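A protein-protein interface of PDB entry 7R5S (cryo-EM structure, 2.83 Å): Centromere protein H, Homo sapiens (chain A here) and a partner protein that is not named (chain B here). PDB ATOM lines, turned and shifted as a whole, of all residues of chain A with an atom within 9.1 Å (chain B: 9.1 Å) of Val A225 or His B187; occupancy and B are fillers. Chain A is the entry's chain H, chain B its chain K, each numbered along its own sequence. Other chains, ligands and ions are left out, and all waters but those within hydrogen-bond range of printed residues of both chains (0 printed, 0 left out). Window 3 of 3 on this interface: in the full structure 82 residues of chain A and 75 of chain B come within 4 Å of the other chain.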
ATOM      1  N   PHE A 216      27.317  21.252  24.711  1.00  0.00           N
ATOM      2  CA  PHE A 216      26.541  20.022  24.601  1.00  0.00           C
ATOM      3  C   PHE A 216      27.390  18.802  24.934  1.00  0.00           C
ATOM      4  O   PHE A 216      26.919  17.875  25.606  1.00  0.00           O
ATOM      5  CB  PHE A 216      25.952  19.896  23.195  1.00  0.00           C
ATOM      6  CG  PHE A 216      24.716  19.042  23.126  1.00  0.00           C
ATOM      7  CD1 PHE A 216      24.150  18.516  24.276  1.00  0.00           C
ATOM      8  CD2 PHE A 216      24.121  18.763  21.908  1.00  0.00           C
ATOM      9  CE1 PHE A 216      23.015  17.731  24.212  1.00  0.00           C
ATOM     10  CE2 PHE A 216      22.986  17.978  21.837  1.00  0.00           C
ATOM     11  CZ  PHE A 216      22.433  17.461  22.991  1.00  0.00           C
ATOM     12  N   GLN A 217      28.643  18.783  24.477  1.00  0.00           N
ATOM     13  CA  GLN A 217      29.518  17.654  24.782  1.00  0.00           C
ATOM     14  C   GLN A 217      29.750  17.533  26.283  1.00  0.00           C
ATOM     15  O   GLN A 217      29.651  16.439  26.853  1.00  0.00           O
ATOM     16  CB  GLN A 217      30.847  17.801  24.040  1.00  0.00           C
ATOM     17  CG  GLN A 217      31.791  16.626  24.236  1.00  0.00           C
ATOM     18  CD  GLN A 217      33.144  16.852  23.592  1.00  0.00           C
ATOM     19  OE1 GLN A 217      33.516  17.984  23.286  1.00  0.00           O
ATOM     20  NE2 GLN A 217      33.885  15.772  23.381  1.00  0.00           N
ATOM     21  N   LEU A 219      27.864  18.683  28.693  1.00  0.00           N
ATOM     22  CA  LEU A 219      26.620  18.307  29.356  1.00  0.00           C
ATOM     23  C   LEU A 219      26.342  16.817  29.214  1.00  0.00           C
ATOM     24  O   LEU A 219      25.958  16.155  30.186  1.00  0.00           O
ATOM     25  CB  LEU A 219      25.456  19.121  28.794  1.00  0.00           C
ATOM     26  CG  LEU A 219      25.082  20.395  29.552  1.00  0.00           C
ATOM     27  CD1 LEU A 219      23.867  21.048  28.915  1.00  0.00           C
ATOM     28  CD2 LEU A 219      24.823  20.089  31.018  1.00  0.00           C
ATOM     29  N   ILE A 220      26.522  16.271  28.008  1.00  0.00           N
ATOM     30  CA  ILE A 220      26.297  14.842  27.799  1.00  0.00           C
ATOM     31  C   ILE A 220      27.289  14.024  28.616  1.00  0.00           C
ATOM     32  O   ILE A 220      26.954  12.954  29.139  1.00  0.00           O
ATOM     33  CB  ILE A 220      26.371  14.505  26.298  1.00  0.00           C
ATOM     34  CG1 ILE A 220      25.206  15.158  25.553  1.00  0.00           C
ATOM     35  CG2 ILE A 220      26.362  13.001  26.076  1.00  0.00           C
ATOM     36  CD1 ILE A 220      25.178  14.854  24.074  1.00  0.00           C
ATOM     37  N   LEU A 221      28.520  14.521  28.755  1.00  0.00           N
ATOM     38  CA  LEU A 221      29.508  13.820  29.570  1.00  0.00           C
ATOM     39  C   LEU A 221      29.115  13.828  31.044  1.00  0.00           C
ATOM     40  O   LEU A 221      29.167  12.792  31.716  1.00  0.00           O
ATOM     41  CB  LEU A 221      30.886  14.453  29.380  1.00  0.00           C
ATOM     42  CG  LEU A 221      31.945  14.038  30.402  1.00  0.00           C
ATOM     43  CD1 LEU A 221      32.569  12.702  30.027  1.00  0.00           C
ATOM     44  CD2 LEU A 221      33.001  15.118  30.542  1.00  0.00           C
ATOM     45  N   GLY A 222      28.719  14.993  31.564  1.00  0.00           N
ATOM     46  CA  GLY A 222      28.411  15.112  32.978  1.00  0.00           C
ATOM     47  C   GLY A 222      27.072  14.544  33.391  1.00  0.00           C
ATOM     48  O   GLY A 222      26.858  14.305  34.584  1.00  0.00           O
ATOM     49  N   SER A 223      26.164  14.324  32.439  1.00  0.00           N
ATOM     50  CA  SER A 223      24.857  13.774  32.777  1.00  0.00           C
ATOM     51  C   SER A 223      24.916  12.300  33.158  1.00  0.00           C
ATOM     52  O   SER A 223      23.949  11.797  33.743  1.00  0.00           O
ATOM     53  CB  SER A 223      23.890  13.967  31.609  1.00  0.00           C
ATOM     54  OG  SER A 223      23.985  12.896  30.687  1.00  0.00           O
ATOM     55  N   LYS A 224      26.013  11.608  32.846  1.00  0.00           N
ATOM     56  CA  LYS A 224      26.198  10.195  33.176  1.00  0.00           C
ATOM     57  C   LYS A 224      25.065   9.340  32.604  1.00  0.00           C
ATOM     58  O   LYS A 224      24.332   8.660  33.325  1.00  0.00           O
ATOM     59  CB  LYS A 224      26.332   9.998  34.690  1.00  0.00           C
ATOM     60  CG  LYS A 224      27.696  10.372  35.246  1.00  0.00           C
ATOM     61  CD  LYS A 224      27.860   9.885  36.676  1.00  0.00           C
ATOM     62  CE  LYS A 224      29.259  10.167  37.198  1.00  0.00           C
ATOM     63  NZ  LYS A 224      29.460   9.624  38.571  1.00  0.00           N
ATOM     64  N   VAL A 225      24.936   9.388  31.281  1.00  0.00           N
ATOM     65  CA  VAL A 225      23.929   8.620  30.561  1.00  0.00           C
ATOM     66  C   VAL A 225      24.627   7.795  29.489  1.00  0.00           C
ATOM     67  O   VAL A 225      25.692   8.167  28.985  1.00  0.00           O
ATOM     68  CB  VAL A 225      22.842   9.531  29.943  1.00  0.00           C
ATOM     69  CG1 VAL A 225      23.405  10.335  28.779  1.00  0.00           C
ATOM     70  CG2 VAL A 225      21.626   8.719  29.515  1.00  0.00           C
ATOM     71  N   ASN A 226      24.028   6.655  29.153  1.00  0.00           N
ATOM     72  CA  ASN A 226      24.557   5.768  28.122  1.00  0.00           C
ATOM     73  C   ASN A 226      23.992   6.202  26.775  1.00  0.00           C
ATOM     74  O   ASN A 226      22.805   6.003  26.497  1.00  0.00           O
ATOM     75  CB  ASN A 226      24.205   4.316  28.428  1.00  0.00           C
ATOM     76  CG  ASN A 226      25.166   3.335  27.789  1.00  0.00           C
ATOM     77  OD1 ASN A 226      25.800   3.638  26.779  1.00  0.00           O
ATOM     78  ND2 ASN A 226      25.280   2.149  28.375  1.00  0.00           N
ATOM     79  N   TRP A 227      24.843   6.794  25.936  1.00  0.00           N
ATOM     80  CA  TRP A 227      24.405   7.311  24.646  1.00  0.00           C
ATOM     81  C   TRP A 227      24.541   6.303  23.515  1.00  0.00           C
ATOM     82  O   TRP A 227      23.938   6.502  22.453  1.00  0.00           O
ATOM     83  CB  TRP A 227      25.190   8.579  24.290  1.00  0.00           C
ATOM     84  CG  TRP A 227      26.638   8.524  24.667  1.00  0.00           C
ATOM     85  CD1 TRP A 227      27.201   8.976  25.824  1.00  0.00           C
ATOM     86  CD2 TRP A 227      27.710   7.993  23.879  1.00  0.00           C
ATOM     87  NE1 TRP A 227      28.558   8.756  25.808  1.00  0.00           N
ATOM     88  CE2 TRP A 227      28.896   8.154  24.625  1.00  0.00           C
ATOM     89  CE3 TRP A 227      27.784   7.395  22.618  1.00  0.00           C
ATOM     90  CZ2 TRP A 227      30.138   7.740  24.150  1.00  0.00           C
ATOM     91  CZ3 TRP A 227      29.019   6.985  22.149  1.00  0.00           C
ATOM     92  CH2 TRP A 227      30.178   7.159  22.913  1.00  0.00           C
ATOM     93  N   ALA A 228      25.313   5.231  23.709  1.00  0.00           N
ATOM     94  CA  ALA A 228      25.483   4.240  22.654  1.00  0.00           C
ATOM     95  C   ALA A 228      24.211   3.443  22.393  1.00  0.00           C
ATOM     96  O   ALA A 228      24.037   2.925  21.285  1.00  0.00           O
ATOM     97  CB  ALA A 228      26.628   3.288  23.003  1.00  0.00           C
ATOM     98  N   GLU A 229      23.322   3.333  23.381  1.00  0.00           N
ATOM     99  CA  GLU A 229      22.083   2.589  23.179  1.00  0.00           C
ATOM    100  C   GLU A 229      21.097   3.356  22.307  1.00  0.00           C
ATOM    101  O   GLU A 229      20.356   2.743  21.529  1.00  0.00           O
ATOM    102  CB  GLU A 229      21.448   2.248  24.527  1.00  0.00           C
ATOM    103  CG  GLU A 229      21.820   0.872  25.064  1.00  0.00           C
ATOM    104  CD  GLU A 229      23.319   0.661  25.158  1.00  0.00           C
ATOM    105  OE1 GLU A 229      24.033   1.604  25.556  1.00  0.00           O
ATOM    106  OE2 GLU A 229      23.784  -0.452  24.834  1.00  0.00           O
ATOM    107  N   ASP A 230      21.072   4.684  22.417  1.00  0.00           N
ATOM    108  CA  ASP A 230      20.167   5.499  21.622  1.00  0.00           C
ATOM    109  C   ASP A 230      20.903   6.022  20.400  1.00  0.00           C
ATOM    110  O   ASP A 230      21.802   6.864  20.546  1.00  0.00           O
ATOM    111  CB  ASP A 230      19.617   6.659  22.450  1.00  0.00           C
ATOM    112  CG  ASP A 230      18.620   7.502  21.682  1.00  0.00           C
ATOM    113  OD1 ASP A 230      17.513   7.001  21.393  1.00  0.00           O
ATOM    114  OD2 ASP A 230      18.942   8.668  21.368  1.00  0.00           O
ATOM    115  N   LEU A 233      20.933   9.995  19.747  1.00  0.00           N
ATOM    116  CA  LEU A 233      21.957  10.748  20.461  1.00  0.00           C
ATOM    117  C   LEU A 233      23.358  10.345  20.020  1.00  0.00           C
ATOM    118  O   LEU A 233      24.296  11.142  20.143  1.00  0.00           O
ATOM    119  CB  LEU A 233      21.795  10.550  21.969  1.00  0.00           C
ATOM    120  CG  LEU A 233      22.583  11.482  22.890  1.00  0.00           C
ATOM    121  CD1 LEU A 233      22.148  12.924  22.690  1.00  0.00           C
ATOM    122  CD2 LEU A 233      22.413  11.066  24.342  1.00  0.00           C
ATOM    123  N   VAL A 237      26.495  12.854  19.246  1.00  0.00           N
ATOM    124  CA  VAL A 237      27.781  12.786  19.934  1.00  0.00           C
ATOM    125  C   VAL A 237      28.913  12.416  18.984  1.00  0.00           C
ATOM    126  O   VAL A 237      30.082  12.664  19.299  1.00  0.00           O
ATOM    127  CB  VAL A 237      27.733  11.807  21.122  1.00  0.00           C
ATOM    128  CG1 VAL A 237      26.576  12.145  22.047  1.00  0.00           C
ATOM    129  CG2 VAL A 237      27.638  10.373  20.635  1.00  0.00           C
ATOM    130  N   THR B 179      18.254  19.978  19.432  1.00  0.00           N
ATOM    131  CA  THR B 179      18.583  18.741  20.134  1.00  0.00           C
ATOM    132  C   THR B 179      19.041  19.009  21.563  1.00  0.00           C
ATOM    133  O   THR B 179      18.665  18.270  22.482  1.00  0.00           O
ATOM    134  CB  THR B 179      19.659  17.970  19.371  1.00  0.00           C
ATOM    135  OG1 THR B 179      19.359  17.987  17.970  1.00  0.00           O
ATOM    136  CG2 THR B 179      19.722  16.529  19.853  1.00  0.00           C
ATOM    137  N   LEU B 180      19.837  20.062  21.773  1.00  0.00           N
ATOM    138  CA  LEU B 180      20.276  20.403  23.122  1.00  0.00           C
ATOM    139  C   LEU B 180      19.099  20.808  23.999  1.00  0.00           C
ATOM    140  O   LEU B 180      19.027  20.416  25.170  1.00  0.00           O
ATOM    141  CB  LEU B 180      21.317  21.522  23.067  1.00  0.00           C
ATOM    142  CG  LEU B 180      21.631  22.252  24.375  1.00  0.00           C
ATOM    143  CD1 LEU B 180      22.246  21.305  25.395  1.00  0.00           C
ATOM    144  CD2 LEU B 180      22.549  23.437  24.120  1.00  0.00           C
ATOM    145  N   GLY B 181      18.172  21.599  23.455  1.00  0.00           N
ATOM    146  CA  GLY B 181      16.985  21.956  24.214  1.00  0.00           C
ATOM    147  C   GLY B 181      16.148  20.748  24.584  1.00  0.00           C
ATOM    148  O   GLY B 181      15.688  20.625  25.722  1.00  0.00           O
ATOM    149  N   GLU B 182      15.951  19.832  23.631  1.00  0.00           N
ATOM    150  CA  GLU B 182      15.185  18.622  23.919  1.00  0.00           C
ATOM    151  C   GLU B 182      15.866  17.780  24.991  1.00  0.00           C
ATOM    152  O   GLU B 182      15.202  17.245  25.889  1.00  0.00           O
ATOM    153  CB  GLU B 182      14.993  17.809  22.639  1.00  0.00           C
ATOM    154  CG  GLU B 182      14.059  16.615  22.778  1.00  0.00           C
ATOM    155  CD  GLU B 182      12.828  16.924  23.607  1.00  0.00           C
ATOM    156  OE1 GLU B 182      11.915  17.598  23.087  1.00  0.00           O
ATOM    157  OE2 GLU B 182      12.766  16.484  24.775  1.00  0.00           O
ATOM    158  N   PHE B 183      17.194  17.658  24.919  1.00  0.00           N
ATOM    159  CA  PHE B 183      17.924  16.875  25.912  1.00  0.00           C
ATOM    160  C   PHE B 183      17.806  17.502  27.297  1.00  0.00           C
ATOM    161  O   PHE B 183      17.511  16.813  28.282  1.00  0.00           O
ATOM    162  CB  PHE B 183      19.390  16.745  25.497  1.00  0.00           C
ATOM    163  CG  PHE B 183      20.238  15.994  26.484  1.00  0.00           C
ATOM    164  CD1 PHE B 183      20.247  14.609  26.494  1.00  0.00           C
ATOM    165  CD2 PHE B 183      21.031  16.670  27.395  1.00  0.00           C
ATOM    166  CE1 PHE B 183      21.026  13.913  27.398  1.00  0.00           C
ATOM    167  CE2 PHE B 183      21.813  15.980  28.301  1.00  0.00           C
ATOM    168  CZ  PHE B 183      21.811  14.600  28.303  1.00  0.00           C
ATOM    169  N   LEU B 184      18.029  18.817  27.389  1.00  0.00           N
ATOM    170  CA  LEU B 184      17.942  19.494  28.679  1.00  0.00           C
ATOM    171  C   LEU B 184      16.526  19.468  29.235  1.00  0.00           C
ATOM    172  O   LEU B 184      16.342  19.501  30.457  1.00  0.00           O
ATOM    173  CB  LEU B 184      18.432  20.937  28.549  1.00  0.00           C
ATOM    174  CG  LEU B 184      19.929  21.165  28.764  1.00  0.00           C
ATOM    175  CD1 LEU B 184      20.273  22.635  28.589  1.00  0.00           C
ATOM    176  CD2 LEU B 184      20.350  20.674  30.138  1.00  0.00           C
ATOM    177  N   GLU B 185      15.516  19.412  28.366  1.00  0.00           N
ATOM    178  CA  GLU B 185      14.143  19.354  28.852  1.00  0.00           C
ATOM    179  C   GLU B 185      13.776  17.960  29.344  1.00  0.00           C
ATOM    180  O   GLU B 185      13.145  17.820  30.397  1.00  0.00           O
ATOM    181  CB  GLU B 185      13.178  19.803  27.754  1.00  0.00           C
ATOM    182  CG  GLU B 185      11.716  19.508  28.052  1.00  0.00           C
ATOM    183  CD  GLU B 185      11.227  20.180  29.321  1.00  0.00           C
ATOM    184  OE1 GLU B 185      11.704  21.292  29.633  1.00  0.00           O
ATOM    185  OE2 GLU B 185      10.365  19.594  30.010  1.00  0.00           O
ATOM    186  N   ASP B 186      14.163  16.917  28.607  1.00  0.00           N
ATOM    187  CA  ASP B 186      13.750  15.569  28.977  1.00  0.00           C
ATOM    188  C   ASP B 186      14.622  14.956  30.065  1.00  0.00           C
ATOM    189  O   ASP B 186      14.181  14.012  30.729  1.00  0.00           O
ATOM    190  CB  ASP B 186      13.749  14.653  27.751  1.00  0.00           C
ATOM    191  CG  ASP B 186      15.072  13.944  27.551  1.00  0.00           C
ATOM    192  OD1 ASP B 186      15.130  12.718  27.779  1.00  0.00           O
ATOM    193  OD2 ASP B 186      16.056  14.611  27.170  1.00  0.00           O
ATOM    194  N   HIS B 187      15.839  15.461  30.268  1.00  0.00           N
ATOM    195  CA  HIS B 187      16.737  14.884  31.261  1.00  0.00           C
ATOM    196  C   HIS B 187      16.804  15.675  32.560  1.00  0.00           C
ATOM    197  O   HIS B 187      17.063  15.084  33.614  1.00  0.00           O
ATOM    198  CB  HIS B 187      18.151  14.751  30.684  1.00  0.00           C
ATOM    199  CG  HIS B 187      18.452  13.390  30.139  1.00  0.00           C
ATOM    200  ND1 HIS B 187      19.150  12.440  30.853  1.00  0.00           N
ATOM    201  CD2 HIS B 187      18.145  12.817  28.952  1.00  0.00           C
ATOM    202  CE1 HIS B 187      19.264  11.343  30.127  1.00  0.00           C
ATOM    203  NE2 HIS B 187      18.663  11.545  28.969  1.00  0.00           N
ATOM    204  N   PHE B 188      16.579  16.987  32.522  1.00  0.00           N
ATOM    205  CA  PHE B 188      16.657  17.843  33.705  1.00  0.00           C
ATOM    206  C   PHE B 188      15.383  18.671  33.804  1.00  0.00           C
ATOM    207  O   PHE B 188      15.355  19.843  33.403  1.00  0.00           O
ATOM    208  CB  PHE B 188      17.894  18.740  33.659  1.00  0.00           C
ATOM    209  CG  PHE B 188      19.183  18.007  33.900  1.00  0.00           C
ATOM    210  CD1 PHE B 188      19.853  17.395  32.855  1.00  0.00           C
ATOM    211  CD2 PHE B 188      19.724  17.933  35.172  1.00  0.00           C
ATOM    212  CE1 PHE B 188      21.038  16.721  33.075  1.00  0.00           C
ATOM    213  CE2 PHE B 188      20.908  17.260  35.398  1.00  0.00           C
ATOM    214  CZ  PHE B 188      21.567  16.653  34.347  1.00  0.00           C
ATOM    215  N   PRO B 189      14.304  18.094  34.339  1.00  0.00           N
ATOM    216  CA  PRO B 189      13.055  18.853  34.483  1.00  0.00           C
ATOM    217  C   PRO B 189      13.146  19.929  35.553  1.00  0.00           C
ATOM    218  O   PRO B 189      14.205  20.128  36.158  1.00  0.00           O
ATOM    219  CB  PRO B 189      12.026  17.776  34.859  1.00  0.00           C
ATOM    220  CG  PRO B 189      12.687  16.461  34.547  1.00  0.00           C
ATOM    221  CD  PRO B 189      14.146  16.692  34.752  1.00  0.00           C
ATOM    222  N   LEU B 190      12.044  20.626  35.792  1.00  0.00           N
ATOM    223  CA  LEU B 190      12.023  21.659  36.820  1.00  0.00           C
ATOM    224  C   LEU B 190      12.126  21.017  38.200  1.00  0.00           C
ATOM    225  O   LEU B 190      11.315  20.147  38.535  1.00  0.00           O
ATOM    226  CB  LEU B 190      10.744  22.487  36.716  1.00  0.00           C
ATOM    227  CG  LEU B 190      10.581  23.635  37.716  1.00  0.00           C
ATOM    228  CD1 LEU B 190      11.627  24.712  37.480  1.00  0.00           C
ATOM    229  CD2 LEU B 190       9.179  24.218  37.639  1.00  0.00           C
ATOM    230  N   LEU B 212      18.000  24.724  34.459  1.00  0.00           N
ATOM    231  CA  LEU B 212      19.395  24.841  34.053  1.00  0.00           C
ATOM    232  C   LEU B 212      19.526  25.470  32.671  1.00  0.00           C
ATOM    233  O   LEU B 212      20.532  26.131  32.383  1.00  0.00           O
ATOM    234  CB  LEU B 212      20.062  23.465  34.080  1.00  0.00           C
ATOM    235  CG  LEU B 212      21.552  23.390  33.747  1.00  0.00           C
ATOM    236  CD1 LEU B 212      22.368  24.207  34.736  1.00  0.00           C
ATOM    237  CD2 LEU B 212      22.021  21.943  33.729  1.00  0.00           C
ATOM    238  N   TYR B 242      22.973  22.670  40.715  1.00  0.00           N
ATOM    239  CA  TYR B 242      23.277  22.968  39.317  1.00  0.00           C
ATOM    240  C   TYR B 242      24.595  23.721  39.181  1.00  0.00           C
ATOM    241  O   TYR B 242      25.362  23.478  38.239  1.00  0.00           O
ATOM    242  CB  TYR B 242      22.136  23.767  38.686  1.00  0.00           C
ATOM    243  CG  TYR B 242      20.890  22.957  38.417  1.00  0.00           C
ATOM    244  CD1 TYR B 242      20.903  21.571  38.512  1.00  0.00           C
ATOM    245  CD2 TYR B 242      19.698  23.577  38.064  1.00  0.00           C
ATOM    246  CE1 TYR B 242      19.766  20.827  38.267  1.00  0.00           C
ATOM    247  CE2 TYR B 242      18.556  22.840  37.818  1.00  0.00           C
ATOM    248  CZ  TYR B 242      18.595  21.466  37.921  1.00  0.00           C
ATOM    249  OH  TYR B 242      17.459  20.730  37.675  1.00  0.00           O
ATOM    250  N   LEU B 245      27.312  21.221  39.530  1.00  0.00           N
ATOM    251  CA  LEU B 245      27.397  20.424  38.310  1.00  0.00           C
ATOM    252  C   LEU B 245      28.159  21.171  37.222  1.00  0.00           C
ATOM    253  O   LEU B 245      29.072  20.620  36.590  1.00  0.00           O
ATOM    254  CB  LEU B 245      25.993  20.054  37.829  1.00  0.00           C
ATOM    255  CG  LEU B 245      25.902  19.201  36.563  1.00  0.00           C
ATOM    256  CD1 LEU B 245      26.388  17.787  36.833  1.00  0.00           C
ATOM    257  CD2 LEU B 245      24.480  19.189  36.025  1.00  0.00           C
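Hydrophobic or aromatic side chains of chain A that line the printed part of chain B: Phe A216, Leu A219 and Val A225.
Of the 15 printed residues of chain B, 5 touch a printed residue of chain A.
Printed residues of chain B that touch a printed residue of chain A: Thr B179, Leu B180, Phe B183, Leu B184 and His B187.
Hydrophobic or aromatic side chains of chain B within 4 Å of the printed part of chain A: Leu B180, Phe B183, Leu B184 and His B187.
Among the printed residues, 7 pairs touch across the chains.
O of Ile A220 is in hydrogen-bond range of OG of Ser A223 (3.3 Å).
CZ of Phe A216 touches O of Thr B179 (3.9 Å).
Phe A216 touches Leu B180.
CD2 of Phe B183 touches CE1 of Phe A216 (3.9 Å).
Leu A219 touches Leu B180 (CD1 to CD1, 3.9 Å).
Leu A219 touches Leu B184.
Ser A223 touches Phe B183.
Val A225 touches His B187 (CG2 to CE1, 3.6 Å).
Val A225 touches just one residue of chain B: His B187.
Printed residues of chain A within 4 Å of His B187: Val A225 (3.6 Å).
No residue of chain A comes within 4 Å of Phe B188.
Printed residues of chain B within 4 Å of Leu A219: Leu B180 and Leu B184.
Of the printed residues of chain A, Phe B183 touches Phe A216 (3.9 Å) and Ser A223 (3.6 Å).
Of the printed residues of chain A, Leu B184 touches Leu A219.
Printed residues of chain A within 4 Å of Leu B180: Phe A216 (3.6 Å) and Leu A219 (3.9 Å).
Of the printed residues of chain B, Ser A223 touches Phe B183 (3.6 Å).
Gly B181 touches none of the printed residues of chain A.
Leu B245 touches none of the printed residues of chain A.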
